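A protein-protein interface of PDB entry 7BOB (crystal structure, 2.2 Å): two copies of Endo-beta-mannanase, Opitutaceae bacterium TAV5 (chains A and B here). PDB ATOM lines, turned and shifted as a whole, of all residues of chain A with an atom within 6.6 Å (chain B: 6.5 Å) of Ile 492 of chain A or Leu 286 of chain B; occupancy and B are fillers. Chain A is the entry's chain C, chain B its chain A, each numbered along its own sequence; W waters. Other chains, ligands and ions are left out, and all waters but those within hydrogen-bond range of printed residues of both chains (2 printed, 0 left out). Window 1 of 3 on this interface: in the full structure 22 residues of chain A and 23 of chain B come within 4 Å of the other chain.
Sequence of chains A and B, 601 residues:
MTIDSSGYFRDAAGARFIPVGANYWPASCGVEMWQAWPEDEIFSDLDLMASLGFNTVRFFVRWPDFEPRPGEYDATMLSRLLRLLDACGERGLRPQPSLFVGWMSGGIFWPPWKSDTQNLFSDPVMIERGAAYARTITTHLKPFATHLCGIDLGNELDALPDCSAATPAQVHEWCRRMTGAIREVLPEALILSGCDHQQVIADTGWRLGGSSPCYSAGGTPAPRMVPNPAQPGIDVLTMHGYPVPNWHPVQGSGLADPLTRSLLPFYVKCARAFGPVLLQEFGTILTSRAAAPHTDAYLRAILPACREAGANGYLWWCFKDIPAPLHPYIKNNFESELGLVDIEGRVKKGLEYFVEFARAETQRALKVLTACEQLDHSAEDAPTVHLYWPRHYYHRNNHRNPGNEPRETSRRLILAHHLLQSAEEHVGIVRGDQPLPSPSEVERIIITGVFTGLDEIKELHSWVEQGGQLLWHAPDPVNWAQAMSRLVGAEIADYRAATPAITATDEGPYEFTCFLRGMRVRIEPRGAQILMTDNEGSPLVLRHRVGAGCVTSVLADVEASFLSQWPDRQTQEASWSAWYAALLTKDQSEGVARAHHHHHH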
ATOM      1  N   ASP A 476      -6.904   1.523   9.873  1.00  0.00           N
ATOM      2  CA  ASP A 476      -7.411   0.919  11.098  1.00  0.00           C
ATOM      3  C   ASP A 476      -8.900   1.205  11.289  1.00  0.00           C
ATOM      4  O   ASP A 476      -9.294   2.382  11.372  1.00  0.00           O
ATOM      5  CB  ASP A 476      -6.613   1.435  12.275  1.00  0.00           C
ATOM      6  CG  ASP A 476      -7.217   1.089  13.623  1.00  0.00           C
ATOM      7  OD1 ASP A 476      -7.926   0.073  13.774  1.00  0.00           O
ATOM      8  OD2 ASP A 476      -6.948   1.860  14.561  1.00  0.00           O
ATOM      9  N   PRO A 477      -9.740   0.176  11.417  1.00  0.00           N
ATOM     10  CA  PRO A 477     -11.187   0.405  11.612  1.00  0.00           C
ATOM     11  C   PRO A 477     -11.535   1.247  12.828  1.00  0.00           C
ATOM     12  O   PRO A 477     -12.538   1.968  12.795  1.00  0.00           O
ATOM     13  CB  PRO A 477     -11.753  -1.018  11.759  1.00  0.00           C
ATOM     14  CG  PRO A 477     -10.677  -1.936  11.282  1.00  0.00           C
ATOM     15  CD  PRO A 477      -9.373  -1.249  11.455  1.00  0.00           C
ATOM     16  N   TRP A 480     -11.506   4.639  11.782  1.00  0.00           N
ATOM     17  CA  TRP A 480     -12.142   4.799  10.477  1.00  0.00           C
ATOM     18  C   TRP A 480     -13.488   5.476  10.676  1.00  0.00           C
ATOM     19  O   TRP A 480     -14.518   4.822  10.850  1.00  0.00           O
ATOM     20  CB  TRP A 480     -12.309   3.451   9.788  1.00  0.00           C
ATOM     21  CG  TRP A 480     -12.538   3.613   8.322  1.00  0.00           C
ATOM     22  CD1 TRP A 480     -13.307   4.575   7.710  1.00  0.00           C
ATOM     23  CD2 TRP A 480     -11.980   2.816   7.272  1.00  0.00           C
ATOM     24  NE1 TRP A 480     -13.255   4.416   6.348  1.00  0.00           N
ATOM     25  CE2 TRP A 480     -12.456   3.342   6.052  1.00  0.00           C
ATOM     26  CE3 TRP A 480     -11.134   1.708   7.245  1.00  0.00           C
ATOM     27  CZ2 TRP A 480     -12.104   2.796   4.820  1.00  0.00           C
ATOM     28  CZ3 TRP A 480     -10.779   1.173   6.025  1.00  0.00           C
ATOM     29  CH2 TRP A 480     -11.266   1.713   4.825  1.00  0.00           C
ATOM     30  N   ALA A 481     -13.481   6.807  10.649  1.00  0.00           N
ATOM     31  CA  ALA A 481     -14.711   7.579  10.510  1.00  0.00           C
ATOM     32  C   ALA A 481     -14.595   8.464   9.277  1.00  0.00           C
ATOM     33  O   ALA A 481     -14.056   8.035   8.250  1.00  0.00           O
ATOM     34  CB  ALA A 481     -14.991   8.416  11.762  1.00  0.00           C
ATOM     35  N   SER A 485     -12.236   8.016   5.934  1.00  0.00           N
ATOM     36  CA  SER A 485     -12.982   7.706   4.710  1.00  0.00           C
ATOM     37  C   SER A 485     -12.644   8.669   3.584  1.00  0.00           C
ATOM     38  O   SER A 485     -12.468   8.244   2.441  1.00  0.00           O
ATOM     39  CB  SER A 485     -14.494   7.704   4.959  1.00  0.00           C
ATOM     40  OG  SER A 485     -14.865   6.811   5.989  1.00  0.00           O
ATOM     41  N   ALA A 490     -13.151   5.647   0.723  1.00  0.00           N
ATOM     42  CA  ALA A 490     -14.197   4.631   0.820  1.00  0.00           C
ATOM     43  C   ALA A 490     -14.763   4.638   2.236  1.00  0.00           C
ATOM     44  O   ALA A 490     -14.084   5.028   3.188  1.00  0.00           O
ATOM     45  CB  ALA A 490     -13.663   3.236   0.467  1.00  0.00           C
ATOM     46  N   GLU A 491     -16.007   4.182   2.369  1.00  0.00           N
ATOM     47  CA  GLU A 491     -16.642   4.012   3.669  1.00  0.00           C
ATOM     48  C   GLU A 491     -16.876   2.539   3.951  1.00  0.00           C
ATOM     49  O   GLU A 491     -16.960   1.716   3.037  1.00  0.00           O
ATOM     50  CB  GLU A 491     -17.986   4.738   3.762  1.00  0.00           C
ATOM     51  CG  GLU A 491     -18.055   6.095   3.103  1.00  0.00           C
ATOM     52  CD  GLU A 491     -19.476   6.653   3.058  1.00  0.00           C
ATOM     53  OE1 GLU A 491     -20.448   5.856   3.133  1.00  0.00           O
ATOM     54  OE2 GLU A 491     -19.616   7.892   2.941  1.00  0.00           O
ATOM     55  N   ILE A 492     -17.018   2.221   5.234  1.00  0.00           N
ATOM     56  CA  ILE A 492     -17.281   0.853   5.658  1.00  0.00           C
ATOM     57  C   ILE A 492     -18.766   0.568   5.503  1.00  0.00           C
ATOM     58  O   ILE A 492     -19.603   1.270   6.083  1.00  0.00           O
ATOM     59  CB  ILE A 492     -16.839   0.618   7.106  1.00  0.00           C
ATOM     60  CG1 ILE A 492     -15.329   0.832   7.258  1.00  0.00           C
ATOM     61  CG2 ILE A 492     -17.225  -0.804   7.527  1.00  0.00           C
ATOM     62  CD1 ILE A 492     -14.877   0.976   8.708  1.00  0.00           C
ATOM     63  N   ALA A 493     -19.095  -0.477   4.732  1.00  0.00           N
ATOM     64  CA  ALA A 493     -20.478  -0.920   4.579  1.00  0.00           C
ATOM     65  C   ALA A 493     -20.884  -1.929   5.642  1.00  0.00           C
ATOM     66  O   ALA A 493     -22.066  -2.000   6.001  1.00  0.00           O
ATOM     67  CB  ALA A 493     -20.691  -1.532   3.186  1.00  0.00           C
ATOM     68  N   ASP A 494     -19.928  -2.687   6.170  1.00  0.00           N
ATOM     69  CA  ASP A 494     -20.182  -3.762   7.121  1.00  0.00           C
ATOM     70  C   ASP A 494     -18.838  -4.385   7.485  1.00  0.00           C
ATOM     71  O   ASP A 494     -17.840  -4.184   6.786  1.00  0.00           O
ATOM     72  CB  ASP A 494     -21.129  -4.836   6.537  1.00  0.00           C
ATOM     73  CG  ASP A 494     -21.740  -5.730   7.608  1.00  0.00           C
ATOM     74  OD1 ASP A 494     -21.519  -5.455   8.813  1.00  0.00           O
ATOM     75  OD2 ASP A 494     -22.451  -6.705   7.243  1.00  0.00           O
ATOM     76  N   TYR A 495     -18.821  -5.133   8.586  1.00  0.00           N
ATOM     77  CA  TYR A 495     -17.750  -6.095   8.789  1.00  0.00           C
ATOM     78  C   TYR A 495     -17.999  -7.315   7.899  1.00  0.00           C
ATOM     79  O   TYR A 495     -19.092  -7.505   7.359  1.00  0.00           O
ATOM     80  CB  TYR A 495     -17.666  -6.527  10.257  1.00  0.00           C
ATOM     81  CG  TYR A 495     -17.653  -5.384  11.250  1.00  0.00           C
ATOM     82  CD1 TYR A 495     -16.472  -4.727  11.567  1.00  0.00           C
ATOM     83  CD2 TYR A 495     -18.831  -4.953  11.861  1.00  0.00           C
ATOM     84  CE1 TYR A 495     -16.460  -3.683  12.483  1.00  0.00           C
ATOM     85  CE2 TYR A 495     -18.833  -3.895  12.771  1.00  0.00           C
ATOM     86  CZ  TYR A 495     -17.643  -3.270  13.080  1.00  0.00           C
ATOM     87  OH  TYR A 495     -17.624  -2.222  13.981  1.00  0.00           O
ATOM     88  N   VAL A 521     -13.248  -5.588   7.043  1.00  0.00           N
ATOM     89  CA  VAL A 521     -14.400  -4.749   6.742  1.00  0.00           C
ATOM     90  C   VAL A 521     -14.735  -4.855   5.265  1.00  0.00           C
ATOM     91  O   VAL A 521     -13.862  -5.015   4.411  1.00  0.00           O
ATOM     92  CB  VAL A 521     -14.173  -3.271   7.124  1.00  0.00           C
ATOM     93  CG1 VAL A 521     -14.188  -3.109   8.636  1.00  0.00           C
ATOM     94  CG2 VAL A 521     -12.871  -2.738   6.513  1.00  0.00           C
ATOM     95  N   ARG A 522     -16.022  -4.755   4.972  1.00  0.00           N
ATOM     96  CA  ARG A 522     -16.509  -4.569   3.614  1.00  0.00           C
ATOM     97  C   ARG A 522     -16.620  -3.076   3.336  1.00  0.00           C
ATOM     98  O   ARG A 522     -17.279  -2.350   4.090  1.00  0.00           O
ATOM     99  CB  ARG A 522     -17.859  -5.254   3.461  1.00  0.00           C
ATOM    100  CG  ARG A 522     -18.256  -5.464   2.030  1.00  0.00           C
ATOM    101  CD  ARG A 522     -19.382  -6.492   1.888  1.00  0.00           C
ATOM    102  NE  ARG A 522     -19.007  -7.875   2.208  1.00  0.00           N
ATOM    103  CZ  ARG A 522     -18.229  -8.656   1.453  1.00  0.00           C
ATOM    104  NH1 ARG A 522     -17.687  -8.190   0.328  1.00  0.00           N
ATOM    105  NH2 ARG A 522     -17.987  -9.911   1.833  1.00  0.00           N
ATOM    106  N   ILE A 523     -15.971  -2.606   2.279  1.00  0.00           N
ATOM    107  CA  ILE A 523     -15.975  -1.181   1.976  1.00  0.00           C
ATOM    108  C   ILE A 523     -16.829  -0.932   0.741  1.00  0.00           C
ATOM    109  O   ILE A 523     -17.061  -1.821  -0.079  1.00  0.00           O
ATOM    110  CB  ILE A 523     -14.549  -0.627   1.778  1.00  0.00           C
ATOM    111  CG1 ILE A 523     -13.869  -1.324   0.599  1.00  0.00           C
ATOM    112  CG2 ILE A 523     -13.733  -0.820   3.034  1.00  0.00           C
ATOM    113  CD1 ILE A 523     -13.676  -0.453  -0.620  1.00  0.00           C
ATOM    114  N   GLU A 524     -17.313   0.303   0.620  1.00  0.00           N
ATOM    115  CA  GLU A 524     -17.897   0.784  -0.616  1.00  0.00           C
ATOM    116  C   GLU A 524     -17.133   2.028  -1.049  1.00  0.00           C
ATOM    117  O   GLU A 524     -16.878   2.911  -0.218  1.00  0.00           O
ATOM    118  CB  GLU A 524     -19.397   1.104  -0.466  1.00  0.00           C
ATOM    119  CG  GLU A 524     -20.065   1.294  -1.820  1.00  0.00           C
ATOM    120  CD  GLU A 524     -21.577   1.208  -1.771  1.00  0.00           C
ATOM    121  OE1 GLU A 524     -22.111   0.074  -1.768  1.00  0.00           O
ATOM    122  OE2 GLU A 524     -22.233   2.276  -1.735  1.00  0.00           O
ATOM    123  N   PRO B 243     -22.234  -4.844  17.633  1.00  0.00           N
ATOM    124  CA  PRO B 243     -21.896  -5.947  16.707  1.00  0.00           C
ATOM    125  C   PRO B 243     -20.417  -6.125  16.367  1.00  0.00           C
ATOM    126  O   PRO B 243     -20.094  -7.060  15.627  1.00  0.00           O
ATOM    127  CB  PRO B 243     -22.686  -5.567  15.445  1.00  0.00           C
ATOM    128  CG  PRO B 243     -22.769  -4.043  15.487  1.00  0.00           C
ATOM    129  CD  PRO B 243     -22.848  -3.687  16.947  1.00  0.00           C
ATOM    130  N   LEU B 255     -23.027  -7.095  10.670  1.00  0.00           N
ATOM    131  CA  LEU B 255     -24.432  -6.707  10.761  1.00  0.00           C
ATOM    132  C   LEU B 255     -25.353  -7.748  10.127  1.00  0.00           C
ATOM    133  O   LEU B 255     -26.434  -8.035  10.656  1.00  0.00           O
ATOM    134  CB  LEU B 255     -24.630  -5.354  10.100  1.00  0.00           C
ATOM    135  CG  LEU B 255     -23.946  -4.217  10.840  1.00  0.00           C
ATOM    136  CD1 LEU B 255     -23.801  -3.010   9.930  1.00  0.00           C
ATOM    137  CD2 LEU B 255     -24.708  -3.887  12.107  1.00  0.00           C
ATOM    138  N   GLY B 283     -26.022  -0.234  19.747  1.00  0.00           N
ATOM    139  CA  GLY B 283     -25.638   0.594  18.619  1.00  0.00           C
ATOM    140  C   GLY B 283     -25.146  -0.264  17.484  1.00  0.00           C
ATOM    141  O   GLY B 283     -24.879  -1.453  17.661  1.00  0.00           O
ATOM    142  N   THR B 284     -25.059   0.345  16.303  1.00  0.00           N
ATOM    143  CA  THR B 284     -24.494  -0.384  15.175  1.00  0.00           C
ATOM    144  C   THR B 284     -23.024  -0.092  14.955  1.00  0.00           C
ATOM    145  O   THR B 284     -22.363  -0.872  14.265  1.00  0.00           O
ATOM    146  CB  THR B 284     -25.235  -0.073  13.869  1.00  0.00           C
ATOM    147  OG1 THR B 284     -25.177   1.337  13.623  1.00  0.00           O
ATOM    148  CG2 THR B 284     -26.692  -0.559  13.932  1.00  0.00           C
ATOM    149  N   ILE B 285     -22.507   1.012  15.517  1.00  0.00           N
ATOM    150  CA  ILE B 285     -21.112   1.433  15.378  1.00  0.00           C
ATOM    151  C   ILE B 285     -20.864   1.940  13.963  1.00  0.00           C
ATOM    152  O   ILE B 285     -20.480   3.095  13.759  1.00  0.00           O
ATOM    153  CB  ILE B 285     -20.111   0.309  15.742  1.00  0.00           C
ATOM    154  CG1 ILE B 285     -20.312  -0.138  17.193  1.00  0.00           C
ATOM    155  CG2 ILE B 285     -18.652   0.794  15.500  1.00  0.00           C
ATOM    156  CD1 ILE B 285     -20.041   0.994  18.218  1.00  0.00           C
ATOM    157  N   LEU B 286     -21.029   1.078  12.972  1.00  0.00           N
ATOM    158  CA  LEU B 286     -21.031   1.563  11.600  1.00  0.00           C
ATOM    159  C   LEU B 286     -22.347   2.286  11.376  1.00  0.00           C
ATOM    160  O   LEU B 286     -23.419   1.729  11.660  1.00  0.00           O
ATOM    161  CB  LEU B 286     -20.857   0.409  10.617  1.00  0.00           C
ATOM    162  CG  LEU B 286     -19.725  -0.573  10.945  1.00  0.00           C
ATOM    163  CD1 LEU B 286     -19.784  -1.776  10.006  1.00  0.00           C
ATOM    164  CD2 LEU B 286     -18.327   0.098  10.897  1.00  0.00           C
ATOM    165  N   THR B 287     -22.278   3.551  10.938  1.00  0.00           N
ATOM    166  CA  THR B 287     -23.513   4.284  10.672  1.00  0.00           C
ATOM    167  C   THR B 287     -23.436   5.106   9.386  1.00  0.00           C
ATOM    168  O   THR B 287     -24.257   6.012   9.196  1.00  0.00           O
ATOM    169  CB  THR B 287     -23.885   5.232  11.833  1.00  0.00           C
ATOM    170  OG1 THR B 287     -22.920   6.279  11.912  1.00  0.00           O
ATOM    171  CG2 THR B 287     -23.968   4.511  13.186  1.00  0.00           C
ATOM    172  N   SER B 288     -22.486   4.822   8.499  1.00  0.00           N
ATOM    173  CA  SER B 288     -22.337   5.606   7.282  1.00  0.00           C
ATOM    174  C   SER B 288     -23.444   5.268   6.280  1.00  0.00           C
ATOM    175  O   SER B 288     -24.232   4.336   6.468  1.00  0.00           O
ATOM    176  CB  SER B 288     -20.952   5.384   6.658  1.00  0.00           C
ATOM    177  OG  SER B 288     -20.904   4.194   5.870  1.00  0.00           O
ATOM    178  N   ARG B 289     -23.519   6.081   5.223  1.00  0.00           N
ATOM    179  CA  ARG B 289     -24.504   5.864   4.171  1.00  0.00           C
ATOM    180  C   ARG B 289     -24.334   4.483   3.553  1.00  0.00           C
ATOM    181  O   ARG B 289     -25.315   3.763   3.343  1.00  0.00           O
ATOM    182  CB  ARG B 289     -24.372   6.959   3.109  1.00  0.00           C
ATOM    183  CG  ARG B 289     -25.434   6.936   2.029  1.00  0.00           C
ATOM    184  CD  ARG B 289     -24.836   7.188   0.639  1.00  0.00           C
ATOM    185  NE  ARG B 289     -25.734   6.715  -0.424  1.00  0.00           N
ATOM    186  CZ  ARG B 289     -25.721   5.488  -0.949  1.00  0.00           C
ATOM    187  NH1 ARG B 289     -24.850   4.574  -0.521  1.00  0.00           N
ATOM    188  NH2 ARG B 289     -26.591   5.176  -1.912  1.00  0.00           N
ATOM    189  N   ALA B 290     -23.085   4.070   3.315  1.00  0.00           N
ATOM    190  CA  ALA B 290     -22.838   2.755   2.732  1.00  0.00           C
ATOM    191  C   ALA B 290     -23.364   1.632   3.616  1.00  0.00           C
ATOM    192  O   ALA B 290     -23.764   0.584   3.110  1.00  0.00           O
ATOM    193  CB  ALA B 290     -21.346   2.573   2.471  1.00  0.00           C
ATOM    194  N   ALA B 291     -23.405   1.838   4.931  1.00  0.00           N
ATOM    195  CA  ALA B 291     -23.868   0.796   5.838  1.00  0.00           C
ATOM    196  C   ALA B 291     -25.380   0.733   5.968  1.00  0.00           C
ATOM    197  O   ALA B 291     -25.881  -0.216   6.585  1.00  0.00           O
ATOM    198  CB  ALA B 291     -23.271   0.999   7.234  1.00  0.00           C
ATOM    199  N   THR B 295     -27.350  -1.824   8.468  1.00  0.00           N
ATOM    200  CA  THR B 295     -27.733  -1.429   9.816  1.00  0.00           C
ATOM    201  C   THR B 295     -29.242  -1.518   9.994  1.00  0.00           C
ATOM    202  O   THR B 295     -29.739  -1.899  11.064  1.00  0.00           O
ATOM    203  CB  THR B 295     -27.215  -0.016  10.116  1.00  0.00           C
ATOM    204  OG1 THR B 295     -27.754   0.926   9.173  1.00  0.00           O
ATOM    205  CG2 THR B 295     -25.669  -0.004  10.027  1.00  0.00           C
ATOM    206  N   TRP B 316     -30.250   4.038  22.654  1.00  0.00           N
ATOM    207  CA  TRP B 316     -29.254   3.982  21.604  1.00  0.00           C
ATOM    208  C   TRP B 316     -27.957   4.675  22.030  1.00  0.00           C
ATOM    209  O   TRP B 316     -27.966   5.623  22.820  1.00  0.00           O
ATOM    210  CB  TRP B 316     -29.835   4.627  20.353  1.00  0.00           C
ATOM    211  CG  TRP B 316     -28.852   4.946  19.300  1.00  0.00           C
ATOM    212  CD1 TRP B 316     -28.128   6.096  19.169  1.00  0.00           C
ATOM    213  CD2 TRP B 316     -28.501   4.117  18.195  1.00  0.00           C
ATOM    214  NE1 TRP B 316     -27.350   6.034  18.044  1.00  0.00           N
ATOM    215  CE2 TRP B 316     -27.555   4.824  17.430  1.00  0.00           C
ATOM    216  CE3 TRP B 316     -28.908   2.850  17.769  1.00  0.00           C
ATOM    217  CZ2 TRP B 316     -26.983   4.293  16.271  1.00  0.00           C
ATOM    218  CZ3 TRP B 316     -28.347   2.327  16.614  1.00  0.00           C
ATOM    219  CH2 TRP B 316     -27.403   3.052  15.874  1.00  0.00           C
ATOM    220  N   GLU B 337     -18.645   9.018  15.193  1.00  0.00           N
ATOM    221  CA  GLU B 337     -19.676   8.797  14.173  1.00  0.00           C
ATOM    222  C   GLU B 337     -20.650   7.704  14.613  1.00  0.00           C
ATOM    223  O   GLU B 337     -20.992   6.793  13.858  1.00  0.00           O
ATOM    224  CB  GLU B 337     -19.046   8.446  12.825  1.00  0.00           C
ATOM    225  CG  GLU B 337     -19.976   8.755  11.653  1.00  0.00           C
ATOM    226  CD  GLU B 337     -19.382   8.399  10.300  1.00  0.00           C
ATOM    227  OE1 GLU B 337     -18.146   8.480  10.146  1.00  0.00           O
ATOM    228  OE2 GLU B 337     -20.159   8.046   9.384  1.00  0.00           O
ATOM    229  N   LEU B 338     -21.109   7.787  15.857  1.00  0.00           N
ATOM    230  CA  LEU B 338     -22.086   6.846  16.385  1.00  0.00           C
ATOM    231  C   LEU B 338     -23.484   7.457  16.495  1.00  0.00           C
ATOM    232  O   LEU B 338     -24.381   6.832  17.079  1.00  0.00           O
ATOM    233  CB  LEU B 338     -21.612   6.341  17.745  1.00  0.00           C
ATOM    234  CG  LEU B 338     -20.189   5.743  17.671  1.00  0.00           C
ATOM    235  CD1 LEU B 338     -19.740   5.246  19.026  1.00  0.00           C
ATOM    236  CD2 LEU B 338     -20.143   4.602  16.623  1.00  0.00           C
ATOM    237  N   LEU B 351     -30.998   4.013  10.093  1.00  0.00           N
ATOM    238  CA  LEU B 351     -31.308   3.859  11.510  1.00  0.00           C
ATOM    239  C   LEU B 351     -32.754   4.209  11.871  1.00  0.00           C
ATOM    240  O   LEU B 351     -33.138   4.056  13.043  1.00  0.00           O
ATOM    241  CB  LEU B 351     -30.332   4.707  12.345  1.00  0.00           C
ATOM    242  CG  LEU B 351     -28.819   4.559  12.037  1.00  0.00           C
ATOM    243  CD1 LEU B 351     -27.963   5.365  13.008  1.00  0.00           C
ATOM    244  CD2 LEU B 351     -28.369   3.094  12.014  1.00  0.00           C
HETATM  245  O   HOH W   1     -22.087  -9.327   8.302  1.00  0.00           O
HETATM  246  O   HOH W   2     -20.316   2.741   8.517  1.00  0.00           O
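Water W1 bridges the side-chain carboxylate (OD2) of Asp 494 of chain A (2.9 Å) and the backbone NH (N) of Leu 255 of chain B (3.4 Å).
Water W2 lies within hydrogen-bond range of the backbone carbonyl oxygen (O) of Ile 492 of chain A (2.9 Å), the backbone NH (N) of Ser 288 of chain B (3.0 Å) and the backbone NH (N) of Thr 287 of chain B (3.2 Å).
The backbone carbonyl oxygen (O) of Asp 494 of chain A is in hydrogen-bond range of the backbone NH (N) of Arg 522 of chain A (2.6 Å).
O of Ala 481 of chain A sits at hydrogen-bond distance from OG of Ser 485 of chain A, 2.7 Å away.
O of Glu 491 of chain A sits at hydrogen-bond distance from N of Glu 524 of chain A, at 2.8 Å.
The side-chain hydroxyl (OG1) of Thr 287 of chain B lies within hydrogen-bond range of the backbone carbonyl oxygen (O) of Glu 337 of chain B (2.8 Å).
The side-chain hydroxyl (OG1) of Thr 284 of chain B is in hydrogen-bond range of the backbone carbonyl oxygen (O) of Leu 286 of chain B.
The backbone carbonyl oxygen (O) of Ala 291 of chain B is in hydrogen-bond range of the side-chain hydroxyl (OG1) of Thr 295 of chain B, at 3.4 Å.
N of Leu 255 of chain B is in hydrogen-bond range of OD1 of Asp 494 of chain A.
The backbone NH of Ala 290 of chain B lies within hydrogen-bond range of the side-chain carboxylate of Glu 491 of chain A, at 3.2 Å.
OG of Ser 288 of chain B is in hydrogen-bond range of O of Ile 492 of chain A (3.2 Å).
The guanidinium group of Arg 289 of chain B is in salt-bridge range of the side-chain carboxylate of Glu 524 of chain A (3.7 Å).
OG of Ser 288 of chain B sits at hydrogen-bond distance from OE1 of Glu 491 of chain A, 3.2 Å away.
Of the printed residues of chain B, Ala 481 of chain A touches Glu 337.
Arg 522 of chain A touches none of the printed residues of chain B.
Printed residues of chain A within 4 Å of Ile 285 of chain B: Tyr 495 (3.5 Å).
Of chain A, only Ile 492, Asp 494 and Tyr 495 come within 4 Å of Leu 286 of chain B.
Of the printed residues of chain A, Arg 289 of chain B touches Glu 491 and Glu 524.
Of the printed residues of chain A, Ala 290 of chain B touches Glu 491 (3.2 Å), Ala 493 (3.7 Å) and Glu 524 (3.8 Å).
The nearest residue of chain A that does not touch Leu 286 of chain B is Ala 493 of chain A (4.5 Å).
CB of Ala 481 of chain A touches OE1 of Glu 337 of chain B, 3.5 Å away.
Arg 289 of chain B touches Glu 491 of chain A.
Ile 492 of chain A touches Leu 286 of chain B.
Ala 291 of chain B touches Ile 492 of chain A (CB to O, 3.9 Å).
Ala 493 of chain A touches Ala 290 of chain B.
Ala 291 of chain B touches Ala 493 of chain A.
CD1 of Leu 286 of chain B touches CA of Asp 494 of chain A, at 3.5 Å.
OH of Tyr 495 of chain A touches CG2 of Ile 285 of chain B, at 3.5 Å.
Leu 286 of chain B touches Tyr 495 of chain A.
Ala 290 of chain B touches Glu 524 of chain A (CB to CB, 3.8 Å).
No position is printed for both chains.
Of the 15 pairs that touch across the chains among the printed residues, none has its exchanged pair printed and touching as well.
Of the 16 printed residues of chain B, 8 touch a printed residue of chain A.
Hydrophobic or aromatic side chains of chain B within 4 Å of the printed part of chain A: Leu 255, Ile 285, Leu 286, Ala 290 and Ala 291.
Of the 15 printed residues of chain A, 7 touch a printed residue of chain B.
Hydrophobic or aromatic side chains of chain A within 4 Å of the printed part of chain B: Ala 481, Ile 492, Ala 493 and Tyr 495.
Among the printed residues, 15 pairs touch across the chains.
Among the printed residues, Asp or Glu carboxylates within 4 Å of a Lys or Arg side-chain nitrogen of the other chain: Glu 524 of chain A with Arg 289 of chain B (3.7 Å).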
